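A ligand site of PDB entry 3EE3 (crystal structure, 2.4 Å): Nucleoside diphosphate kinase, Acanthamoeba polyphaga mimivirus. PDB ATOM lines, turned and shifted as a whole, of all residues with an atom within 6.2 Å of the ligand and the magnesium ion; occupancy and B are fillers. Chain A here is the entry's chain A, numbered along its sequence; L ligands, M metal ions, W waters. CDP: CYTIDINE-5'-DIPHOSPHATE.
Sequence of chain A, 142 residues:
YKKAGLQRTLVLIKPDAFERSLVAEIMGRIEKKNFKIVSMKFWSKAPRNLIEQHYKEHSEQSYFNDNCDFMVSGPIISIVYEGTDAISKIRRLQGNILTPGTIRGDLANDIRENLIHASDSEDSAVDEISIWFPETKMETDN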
ATOM      1  N   LYS A  14      19.902 -18.517 -31.836  1.00  0.00           N
ATOM      2  CA  LYS A  14      19.411 -19.495 -30.842  1.00  0.00           C
ATOM      3  C   LYS A  14      17.862 -19.497 -30.640  1.00  0.00           C
ATOM      4  O   LYS A  14      17.184 -18.533 -31.031  1.00  0.00           O
ATOM      5  CB  LYS A  14      20.141 -19.302 -29.508  1.00  0.00           C
ATOM      6  CG  LYS A  14      21.679 -19.365 -29.595  1.00  0.00           C
ATOM      7  CD  LYS A  14      22.312 -19.130 -28.220  1.00  0.00           C
ATOM      8  CE  LYS A  14      23.794 -19.417 -28.202  1.00  0.00           C
ATOM      9  NZ  LYS A  14      24.335 -19.496 -26.800  1.00  0.00           N
ATOM     10  N   TYR A  55      29.538 -27.769 -29.347  1.00  0.00           N
ATOM     11  CA  TYR A  55      29.987 -27.427 -27.993  1.00  0.00           C
ATOM     12  C   TYR A  55      30.910 -28.476 -27.324  1.00  0.00           C
ATOM     13  O   TYR A  55      30.971 -28.543 -26.077  1.00  0.00           O
ATOM     14  CB  TYR A  55      28.782 -27.144 -27.092  1.00  0.00           C
ATOM     15  CG  TYR A  55      28.095 -25.813 -27.325  1.00  0.00           C
ATOM     16  CD1 TYR A  55      26.792 -25.747 -27.850  1.00  0.00           C
ATOM     17  CD2 TYR A  55      28.736 -24.600 -27.015  1.00  0.00           C
ATOM     18  CE1 TYR A  55      26.150 -24.521 -28.057  1.00  0.00           C
ATOM     19  CE2 TYR A  55      28.112 -23.369 -27.224  1.00  0.00           C
ATOM     20  CZ  TYR A  55      26.819 -23.345 -27.748  1.00  0.00           C
ATOM     21  OH  TYR A  55      26.183 -22.139 -27.967  1.00  0.00           O
ATOM     22  N   HIS A  58      33.150 -28.040 -24.442  1.00  0.00           N
ATOM     23  CA  HIS A  58      32.418 -27.760 -23.203  1.00  0.00           C
ATOM     24  C   HIS A  58      31.891 -29.001 -22.458  1.00  0.00           C
ATOM     25  O   HIS A  58      31.197 -28.841 -21.441  1.00  0.00           O
ATOM     26  CB  HIS A  58      31.233 -26.812 -23.475  1.00  0.00           C
ATOM     27  CG  HIS A  58      31.623 -25.423 -23.873  1.00  0.00           C
ATOM     28  ND1 HIS A  58      31.779 -24.400 -22.956  1.00  0.00           N
ATOM     29  CD2 HIS A  58      31.843 -24.877 -25.099  1.00  0.00           C
ATOM     30  CE1 HIS A  58      32.126 -23.289 -23.594  1.00  0.00           C
ATOM     31  NE2 HIS A  58      32.170 -23.556 -24.888  1.00  0.00           N
ATOM     32  N   SER A  62      29.422 -28.449 -15.743  1.00  0.00           N
ATOM     33  CA  SER A  62      28.123 -28.597 -15.085  1.00  0.00           C
ATOM     34  C   SER A  62      26.941 -28.305 -16.028  1.00  0.00           C
ATOM     35  O   SER A  62      25.964 -29.080 -16.066  1.00  0.00           O
ATOM     36  CB  SER A  62      28.036 -27.679 -13.850  1.00  0.00           C
ATOM     37  OG  SER A  62      28.689 -26.439 -14.111  1.00  0.00           O
ATOM     38  N   TYR A  63      27.070 -27.217 -16.786  1.00  0.00           N
ATOM     39  CA  TYR A  63      25.976 -26.675 -17.634  1.00  0.00           C
ATOM     40  C   TYR A  63      25.781 -27.360 -18.982  1.00  0.00           C
ATOM     41  O   TYR A  63      24.800 -27.077 -19.655  1.00  0.00           O
ATOM     42  CB  TYR A  63      26.171 -25.171 -17.852  1.00  0.00           C
ATOM     43  CG  TYR A  63      27.456 -24.802 -18.587  1.00  0.00           C
ATOM     44  CD1 TYR A  63      27.554 -24.932 -19.968  1.00  0.00           C
ATOM     45  CD2 TYR A  63      28.550 -24.319 -17.889  1.00  0.00           C
ATOM     46  CE1 TYR A  63      28.715 -24.594 -20.636  1.00  0.00           C
ATOM     47  CE2 TYR A  63      29.733 -23.974 -18.551  1.00  0.00           C
ATOM     48  CZ  TYR A  63      29.798 -24.113 -19.930  1.00  0.00           C
ATOM     49  OH  TYR A  63      30.960 -23.774 -20.574  1.00  0.00           O
ATOM     50  N   ASP A  66      22.141 -29.259 -19.786  1.00  0.00           N
ATOM     51  CA  ASP A  66      21.106 -28.209 -19.785  1.00  0.00           C
ATOM     52  C   ASP A  66      21.200 -27.256 -21.003  1.00  0.00           C
ATOM     53  O   ASP A  66      20.180 -26.826 -21.535  1.00  0.00           O
ATOM     54  CB  ASP A  66      21.157 -27.371 -18.498  1.00  0.00           C
ATOM     55  CG  ASP A  66      20.914 -28.193 -17.231  1.00  0.00           C
ATOM     56  OD1 ASP A  66      20.041 -29.094 -17.259  1.00  0.00           O
ATOM     57  OD2 ASP A  66      21.605 -27.907 -16.197  1.00  0.00           O
ATOM     58  N   ASN A  67      22.406 -26.908 -21.425  1.00  0.00           N
ATOM     59  CA  ASN A  67      22.555 -26.013 -22.570  1.00  0.00           C
ATOM     60  C   ASN A  67      22.180 -26.706 -23.879  1.00  0.00           C
ATOM     61  O   ASN A  67      21.545 -26.099 -24.754  1.00  0.00           O
ATOM     62  CB  ASN A  67      23.966 -25.422 -22.626  1.00  0.00           C
ATOM     63  CG  ASN A  67      24.135 -24.441 -23.780  1.00  0.00           C
ATOM     64  OD1 ASN A  67      25.136 -24.473 -24.485  1.00  0.00           O
ATOM     65  ND2 ASN A  67      23.141 -23.568 -23.992  1.00  0.00           N
ATOM     66  N   PHE A  70      18.298 -26.924 -24.089  1.00  0.00           N
ATOM     67  CA  PHE A  70      17.814 -25.628 -24.591  1.00  0.00           C
ATOM     68  C   PHE A  70      18.046 -25.479 -26.114  1.00  0.00           C
ATOM     69  O   PHE A  70      17.123 -25.110 -26.851  1.00  0.00           O
ATOM     70  CB  PHE A  70      18.448 -24.492 -23.754  1.00  0.00           C
ATOM     71  CG  PHE A  70      18.493 -23.146 -24.452  1.00  0.00           C
ATOM     72  CD1 PHE A  70      19.735 -22.561 -24.799  1.00  0.00           C
ATOM     73  CD2 PHE A  70      17.314 -22.446 -24.764  1.00  0.00           C
ATOM     74  CE1 PHE A  70      19.796 -21.312 -25.437  1.00  0.00           C
ATOM     75  CE2 PHE A  70      17.384 -21.188 -25.423  1.00  0.00           C
ATOM     76  CZ  PHE A  70      18.617 -20.633 -25.744  1.00  0.00           C
ATOM     77  N   ARG A  91      32.142 -11.028 -33.468  1.00  0.00           N
ATOM     78  CA  ARG A  91      32.234 -11.432 -32.054  1.00  0.00           C
ATOM     79  C   ARG A  91      32.032 -10.237 -31.113  1.00  0.00           C
ATOM     80  O   ARG A  91      31.358 -10.371 -30.099  1.00  0.00           O
ATOM     81  CB  ARG A  91      33.574 -12.144 -31.789  1.00  0.00           C
ATOM     82  CG  ARG A  91      33.802 -12.601 -30.341  1.00  0.00           C
ATOM     83  CD  ARG A  91      33.196 -13.981 -30.007  1.00  0.00           C
ATOM     84  NE  ARG A  91      33.328 -14.272 -28.559  1.00  0.00           N
ATOM     85  CZ  ARG A  91      32.689 -15.230 -27.880  1.00  0.00           C
ATOM     86  NH1 ARG A  91      32.903 -15.365 -26.570  1.00  0.00           N
ATOM     87  NH2 ARG A  91      31.844 -16.078 -28.485  1.00  0.00           N
ATOM     88  N   GLN A  94      28.380  -9.281 -31.056  1.00  0.00           N
ATOM     89  CA  GLN A  94      27.677 -10.205 -30.153  1.00  0.00           C
ATOM     90  C   GLN A  94      27.777  -9.732 -28.708  1.00  0.00           C
ATOM     91  O   GLN A  94      26.782  -9.691 -27.982  1.00  0.00           O
ATOM     92  CB  GLN A  94      28.200 -11.638 -30.311  1.00  0.00           C
ATOM     93  CG  GLN A  94      27.851 -12.561 -29.131  1.00  0.00           C
ATOM     94  CD  GLN A  94      28.791 -13.748 -28.949  1.00  0.00           C
ATOM     95  OE1 GLN A  94      28.818 -14.658 -29.763  1.00  0.00           O
ATOM     96  NE2 GLN A  94      29.544 -13.737 -27.851  1.00  0.00           N
ATOM     97  N   GLY A  95      28.993  -9.348 -28.305  1.00  0.00           N
ATOM     98  CA  GLY A  95      29.261  -8.834 -26.962  1.00  0.00           C
ATOM     99  C   GLY A  95      28.839  -9.762 -25.827  1.00  0.00           C
ATOM    100  O   GLY A  95      28.918 -11.007 -25.935  1.00  0.00           O
ATOM    101  N   ASN A  96      28.410  -9.138 -24.722  1.00  0.00           N
ATOM    102  CA  ASN A  96      27.959  -9.869 -23.543  1.00  0.00           C
ATOM    103  C   ASN A  96      26.791  -9.144 -22.899  1.00  0.00           C
ATOM    104  O   ASN A  96      26.463  -8.011 -23.307  1.00  0.00           O
ATOM    105  CB  ASN A  96      29.097 -10.156 -22.541  1.00  0.00           C
ATOM    106  CG  ASN A  96      29.858  -8.895 -22.143  1.00  0.00           C
ATOM    107  OD1 ASN A  96      29.309  -7.950 -21.583  1.00  0.00           O
ATOM    108  ND2 ASN A  96      31.154  -8.900 -22.401  1.00  0.00           N
ATOM    109  N   ARG A 104      23.934  -8.911 -27.331  1.00  0.00           N
ATOM    110  CA  ARG A 104      23.608  -9.454 -26.008  1.00  0.00           C
ATOM    111  C   ARG A 104      23.402  -8.315 -24.974  1.00  0.00           C
ATOM    112  O   ARG A 104      22.522  -8.410 -24.116  1.00  0.00           O
ATOM    113  CB  ARG A 104      24.706 -10.397 -25.513  1.00  0.00           C
ATOM    114  CG  ARG A 104      24.690 -11.787 -26.122  1.00  0.00           C
ATOM    115  CD  ARG A 104      25.920 -12.580 -25.675  1.00  0.00           C
ATOM    116  NE  ARG A 104      25.938 -13.882 -26.317  1.00  0.00           N
ATOM    117  CZ  ARG A 104      26.770 -14.882 -26.000  1.00  0.00           C
ATOM    118  NH1 ARG A 104      27.670 -14.712 -25.029  1.00  0.00           N
ATOM    119  NH2 ARG A 104      26.700 -16.045 -26.643  1.00  0.00           N
ATOM    120  N   ILE A 111      22.603 -16.232 -18.464  1.00  0.00           N
ATOM    121  CA  ILE A 111      23.848 -16.995 -18.772  1.00  0.00           C
ATOM    122  C   ILE A 111      23.693 -18.030 -19.881  1.00  0.00           C
ATOM    123  O   ILE A 111      24.667 -18.388 -20.531  1.00  0.00           O
ATOM    124  CB  ILE A 111      24.494 -17.760 -17.560  1.00  0.00           C
ATOM    125  CG1 ILE A 111      23.461 -18.108 -16.486  1.00  0.00           C
ATOM    126  CG2 ILE A 111      25.728 -17.018 -16.992  1.00  0.00           C
ATOM    127  CD1 ILE A 111      22.812 -19.488 -16.661  1.00  0.00           C
ATOM    128  N   ARG A 112      22.484 -18.524 -20.083  1.00  0.00           N
ATOM    129  CA  ARG A 112      22.259 -19.596 -21.051  1.00  0.00           C
ATOM    130  C   ARG A 112      21.458 -19.148 -22.290  1.00  0.00           C
ATOM    131  O   ARG A 112      21.844 -19.448 -23.421  1.00  0.00           O
ATOM    132  CB  ARG A 112      21.596 -20.814 -20.372  1.00  0.00           C
ATOM    133  CG  ARG A 112      21.071 -21.904 -21.345  1.00  0.00           C
ATOM    134  CD  ARG A 112      20.763 -23.251 -20.659  1.00  0.00           C
ATOM    135  NE  ARG A 112      21.739 -23.519 -19.597  1.00  0.00           N
ATOM    136  CZ  ARG A 112      21.427 -23.914 -18.371  1.00  0.00           C
ATOM    137  NH1 ARG A 112      20.160 -24.141 -18.043  1.00  0.00           N
ATOM    138  NH2 ARG A 112      22.387 -24.095 -17.471  1.00  0.00           N
ATOM    139  N   GLU A 113      20.337 -18.472 -22.061  1.00  0.00           N
ATOM    140  CA  GLU A 113      19.505 -18.007 -23.164  1.00  0.00           C
ATOM    141  C   GLU A 113      19.984 -16.610 -23.543  1.00  0.00           C
ATOM    142  O   GLU A 113      19.540 -15.586 -22.981  1.00  0.00           O
ATOM    143  CB  GLU A 113      18.043 -18.013 -22.771  1.00  0.00           C
ATOM    144  CG  GLU A 113      17.473 -19.392 -22.518  1.00  0.00           C
ATOM    145  CD  GLU A 113      16.098 -19.349 -21.907  1.00  0.00           C
ATOM    146  OE1 GLU A 113      15.725 -18.272 -21.413  1.00  0.00           O
ATOM    147  OE2 GLU A 113      15.384 -20.369 -21.892  1.00  0.00           O
ATOM    148  N   ASN A 114      20.925 -16.589 -24.484  1.00  0.00           N
ATOM    149  CA  ASN A 114      21.600 -15.361 -24.878  1.00  0.00           C
ATOM    150  C   ASN A 114      21.603 -15.080 -26.391  1.00  0.00           C
ATOM    151  O   ASN A 114      22.498 -14.404 -26.912  1.00  0.00           O
ATOM    152  CB  ASN A 114      23.010 -15.251 -24.243  1.00  0.00           C
ATOM    153  CG  ASN A 114      23.926 -16.421 -24.654  1.00  0.00           C
ATOM    154  OD1 ASN A 114      23.604 -17.209 -25.569  1.00  0.00           O
ATOM    155  ND2 ASN A 114      25.051 -16.536 -23.964  1.00  0.00           N
ATOM    156  N   ILE A 116      22.432 -15.542 -29.361  1.00  0.00           N
ATOM    157  CA  ILE A 116      23.385 -15.689 -30.457  1.00  0.00           C
ATOM    158  C   ILE A 116      24.758 -16.258 -30.068  1.00  0.00           C
ATOM    159  O   ILE A 116      25.288 -15.939 -28.992  1.00  0.00           O
ATOM    160  CB  ILE A 116      23.624 -14.308 -31.160  1.00  0.00           C
ATOM    161  CG1 ILE A 116      24.628 -14.458 -32.307  1.00  0.00           C
ATOM    162  CG2 ILE A 116      24.016 -13.171 -30.119  1.00  0.00           C
ATOM    163  CD1 ILE A 116      24.808 -13.240 -33.057  1.00  0.00           C
ATOM    164  N   HIS A 117      25.305 -17.081 -30.976  1.00  0.00           N
ATOM    165  CA  HIS A 117      26.712 -17.540 -30.950  1.00  0.00           C
ATOM    166  C   HIS A 117      27.495 -17.018 -32.150  1.00  0.00           C
ATOM    167  O   HIS A 117      26.985 -17.012 -33.288  1.00  0.00           O
ATOM    168  CB  HIS A 117      26.765 -19.059 -30.976  1.00  0.00           C
ATOM    169  CG  HIS A 117      28.151 -19.595 -31.187  1.00  0.00           C
ATOM    170  ND1 HIS A 117      28.984 -19.943 -30.138  1.00  0.00           N
ATOM    171  CD2 HIS A 117      28.858 -19.820 -32.329  1.00  0.00           C
ATOM    172  CE1 HIS A 117      30.151 -20.359 -30.631  1.00  0.00           C
ATOM    173  NE2 HIS A 117      30.099 -20.299 -31.948  1.00  0.00           N
ATOM    174  N   ALA A 118      28.746 -16.607 -31.910  1.00  0.00           N
ATOM    175  CA  ALA A 118      29.696 -16.287 -32.990  1.00  0.00           C
ATOM    176  C   ALA A 118      31.038 -16.962 -32.722  1.00  0.00           C
ATOM    177  O   ALA A 118      31.490 -16.975 -31.576  1.00  0.00           O
ATOM    178  CB  ALA A 118      29.888 -14.789 -33.113  1.00  0.00           C
ATOM    179  N   ASP A 120      34.881 -17.511 -32.116  1.00  0.00           N
ATOM    180  CA  ASP A 120      35.842 -16.610 -31.459  1.00  0.00           C
ATOM    181  C   ASP A 120      37.289 -16.678 -31.991  1.00  0.00           C
ATOM    182  O   ASP A 120      38.132 -15.891 -31.539  1.00  0.00           O
ATOM    183  CB  ASP A 120      35.827 -16.813 -29.927  1.00  0.00           C
ATOM    184  CG  ASP A 120      36.442 -18.150 -29.481  1.00  0.00           C
ATOM    185  OD1 ASP A 120      36.898 -18.929 -30.339  1.00  0.00           O
ATOM    186  OD2 ASP A 120      36.457 -18.418 -28.255  1.00  0.00           O
HETATM  187  O3B CDP L   1      31.422 -17.513 -25.516  1.00  0.00           O
HETATM  188  PB  CDP L   1      30.050 -17.323 -24.928  1.00  0.00           P
HETATM  189  O1B CDP L   1      29.909 -15.951 -24.321  1.00  0.00           O
HETATM  190  O2B CDP L   1      28.972 -17.858 -25.834  1.00  0.00           O
HETATM  191  O3A CDP L   1      29.846 -18.228 -23.583  1.00  0.00           O
HETATM  192  PA  CDP L   1      30.822 -19.374 -22.933  1.00  0.00           P
HETATM  193  O1A CDP L   1      31.993 -19.630 -23.879  1.00  0.00           O
HETATM  194  O2A CDP L   1      31.101 -18.906 -21.512  1.00  0.00           O
HETATM  195  O5' CDP L   1      29.846 -20.622 -22.958  1.00  0.00           O
HETATM  196  C5' CDP L   1      29.341 -21.049 -24.223  1.00  0.00           C
HETATM  197  C4' CDP L   1      27.820 -21.105 -24.161  1.00  0.00           C
HETATM  198  O4' CDP L   1      27.486 -22.036 -23.133  1.00  0.00           O
HETATM  199  C3' CDP L   1      27.134 -19.817 -23.712  1.00  0.00           C
HETATM  200  O3' CDP L   1      26.757 -18.974 -24.793  1.00  0.00           O
HETATM  201  C2' CDP L   1      25.901 -20.283 -22.997  1.00  0.00           C
HETATM  202  O2' CDP L   1      24.797 -20.335 -23.899  1.00  0.00           O
HETATM  203  C1' CDP L   1      26.280 -21.678 -22.468  1.00  0.00           C
HETATM  204  N1  CDP L   1      26.430 -21.607 -20.998  1.00  0.00           N
HETATM  205  C2  CDP L   1      25.337 -22.078 -20.186  1.00  0.00           C
HETATM  206  O2  CDP L   1      24.304 -22.578 -20.694  1.00  0.00           O
HETATM  207  N3  CDP L   1      25.397 -22.018 -18.849  1.00  0.00           N
HETATM  208  C4  CDP L   1      26.504 -21.505 -18.260  1.00  0.00           C
HETATM  209  N4  CDP L   1      26.516 -21.486 -16.903  1.00  0.00           N
HETATM  210  C5  CDP L   1      27.584 -21.014 -19.028  1.00  0.00           C
HETATM  211  C6  CDP L   1      27.539 -21.079 -20.427  1.00  0.00           C
HETATM  212 MG    MG M   1      33.006 -18.958 -25.566  1.00  0.00          MG
HETATM  213  O   HOH W   1      31.586 -21.304 -19.743  1.00  0.00           O
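Water W1 bridges the side-chain hydroxyl (OH) of Tyr 63 (2.7 Å) and an oxygen (O2A) of the ligand (3.0 Å).
Merely in contact with the ligand: Tyr 55 (3.8 Å), His 58 (3.6 Å), Tyr 63 (3.4 Å), Asn 67 (3.5 Å) and Ile 111 (3.3 Å). Within 4 Å of the ligand: Lys 14, Tyr 55, His 58, Tyr 63, Asn 67, Arg 91, Arg 104, Ile 111, Arg 112 and Asn 114.
The magnesium ion is bound by O1A of the ligand (2.1 Å) and O3B of the ligand (2.1 Å).
Residues that only touch the magnesium ion: Arg 91 (3.7 Å). Of the 21 residues printed, 1 comes within 4 Å of the magnesium ion.
The guanidinium group (NH2) of Arg 104 lies close to the side-chain amide nitrogen (ND2) of Asn 114 (3.2 Å). The backbone NH (N) of Arg 104 is in hydrogen-bond range of the backbone carbonyl oxygen (O) of Gln 94, 3.0 Å away. The guanidinium group (NH2) of Arg 104 is in hydrogen-bond range of the backbone carbonyl oxygen (O) of Ile 116 (2.7 Å). NH2 of Arg 91 lies close to NE2 of Gln 94, 3.3 Å away. NH2 of Arg 91 is in hydrogen-bond range of O of Ala 118, at 3.2 Å. The side-chain amide oxygen (OD1) of Asn 114 sits at hydrogen-bond distance from the side-chain amino group (NZ) of Lys 14 (2.7 Å). The side-chain amino group (NZ) of Lys 14 lies within hydrogen-bond range of the side-chain hydroxyl (OH) of Tyr 55. The side-chain hydroxyl (OH) of Tyr 63 sits at hydrogen-bond distance from a ring nitrogen (ND1) of His 58.
The guanidinium group (NH1) of Arg 104 lies within salt-bridge range of an oxygen (O1B) of the ligand (2.7 Å). O1B of the ligand lies within salt-bridge range of NH1 of Arg 91. The backbone carbonyl oxygen of Arg 112 lies within hydrogen-bond range of an oxygen (O2') of the ligand. An oxygen (O2) of the ligand is in hydrogen-bond range of the guanidinium group (NE) of Arg 112, 2.9 Å away. An oxygen (O2') of the ligand is in hydrogen-bond range of the side-chain amino group (NZ) of Lys 14, at 3.1 Å. ND2 of Asn 114 sits at hydrogen-bond distance from O3' of the ligand (3.1 Å).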
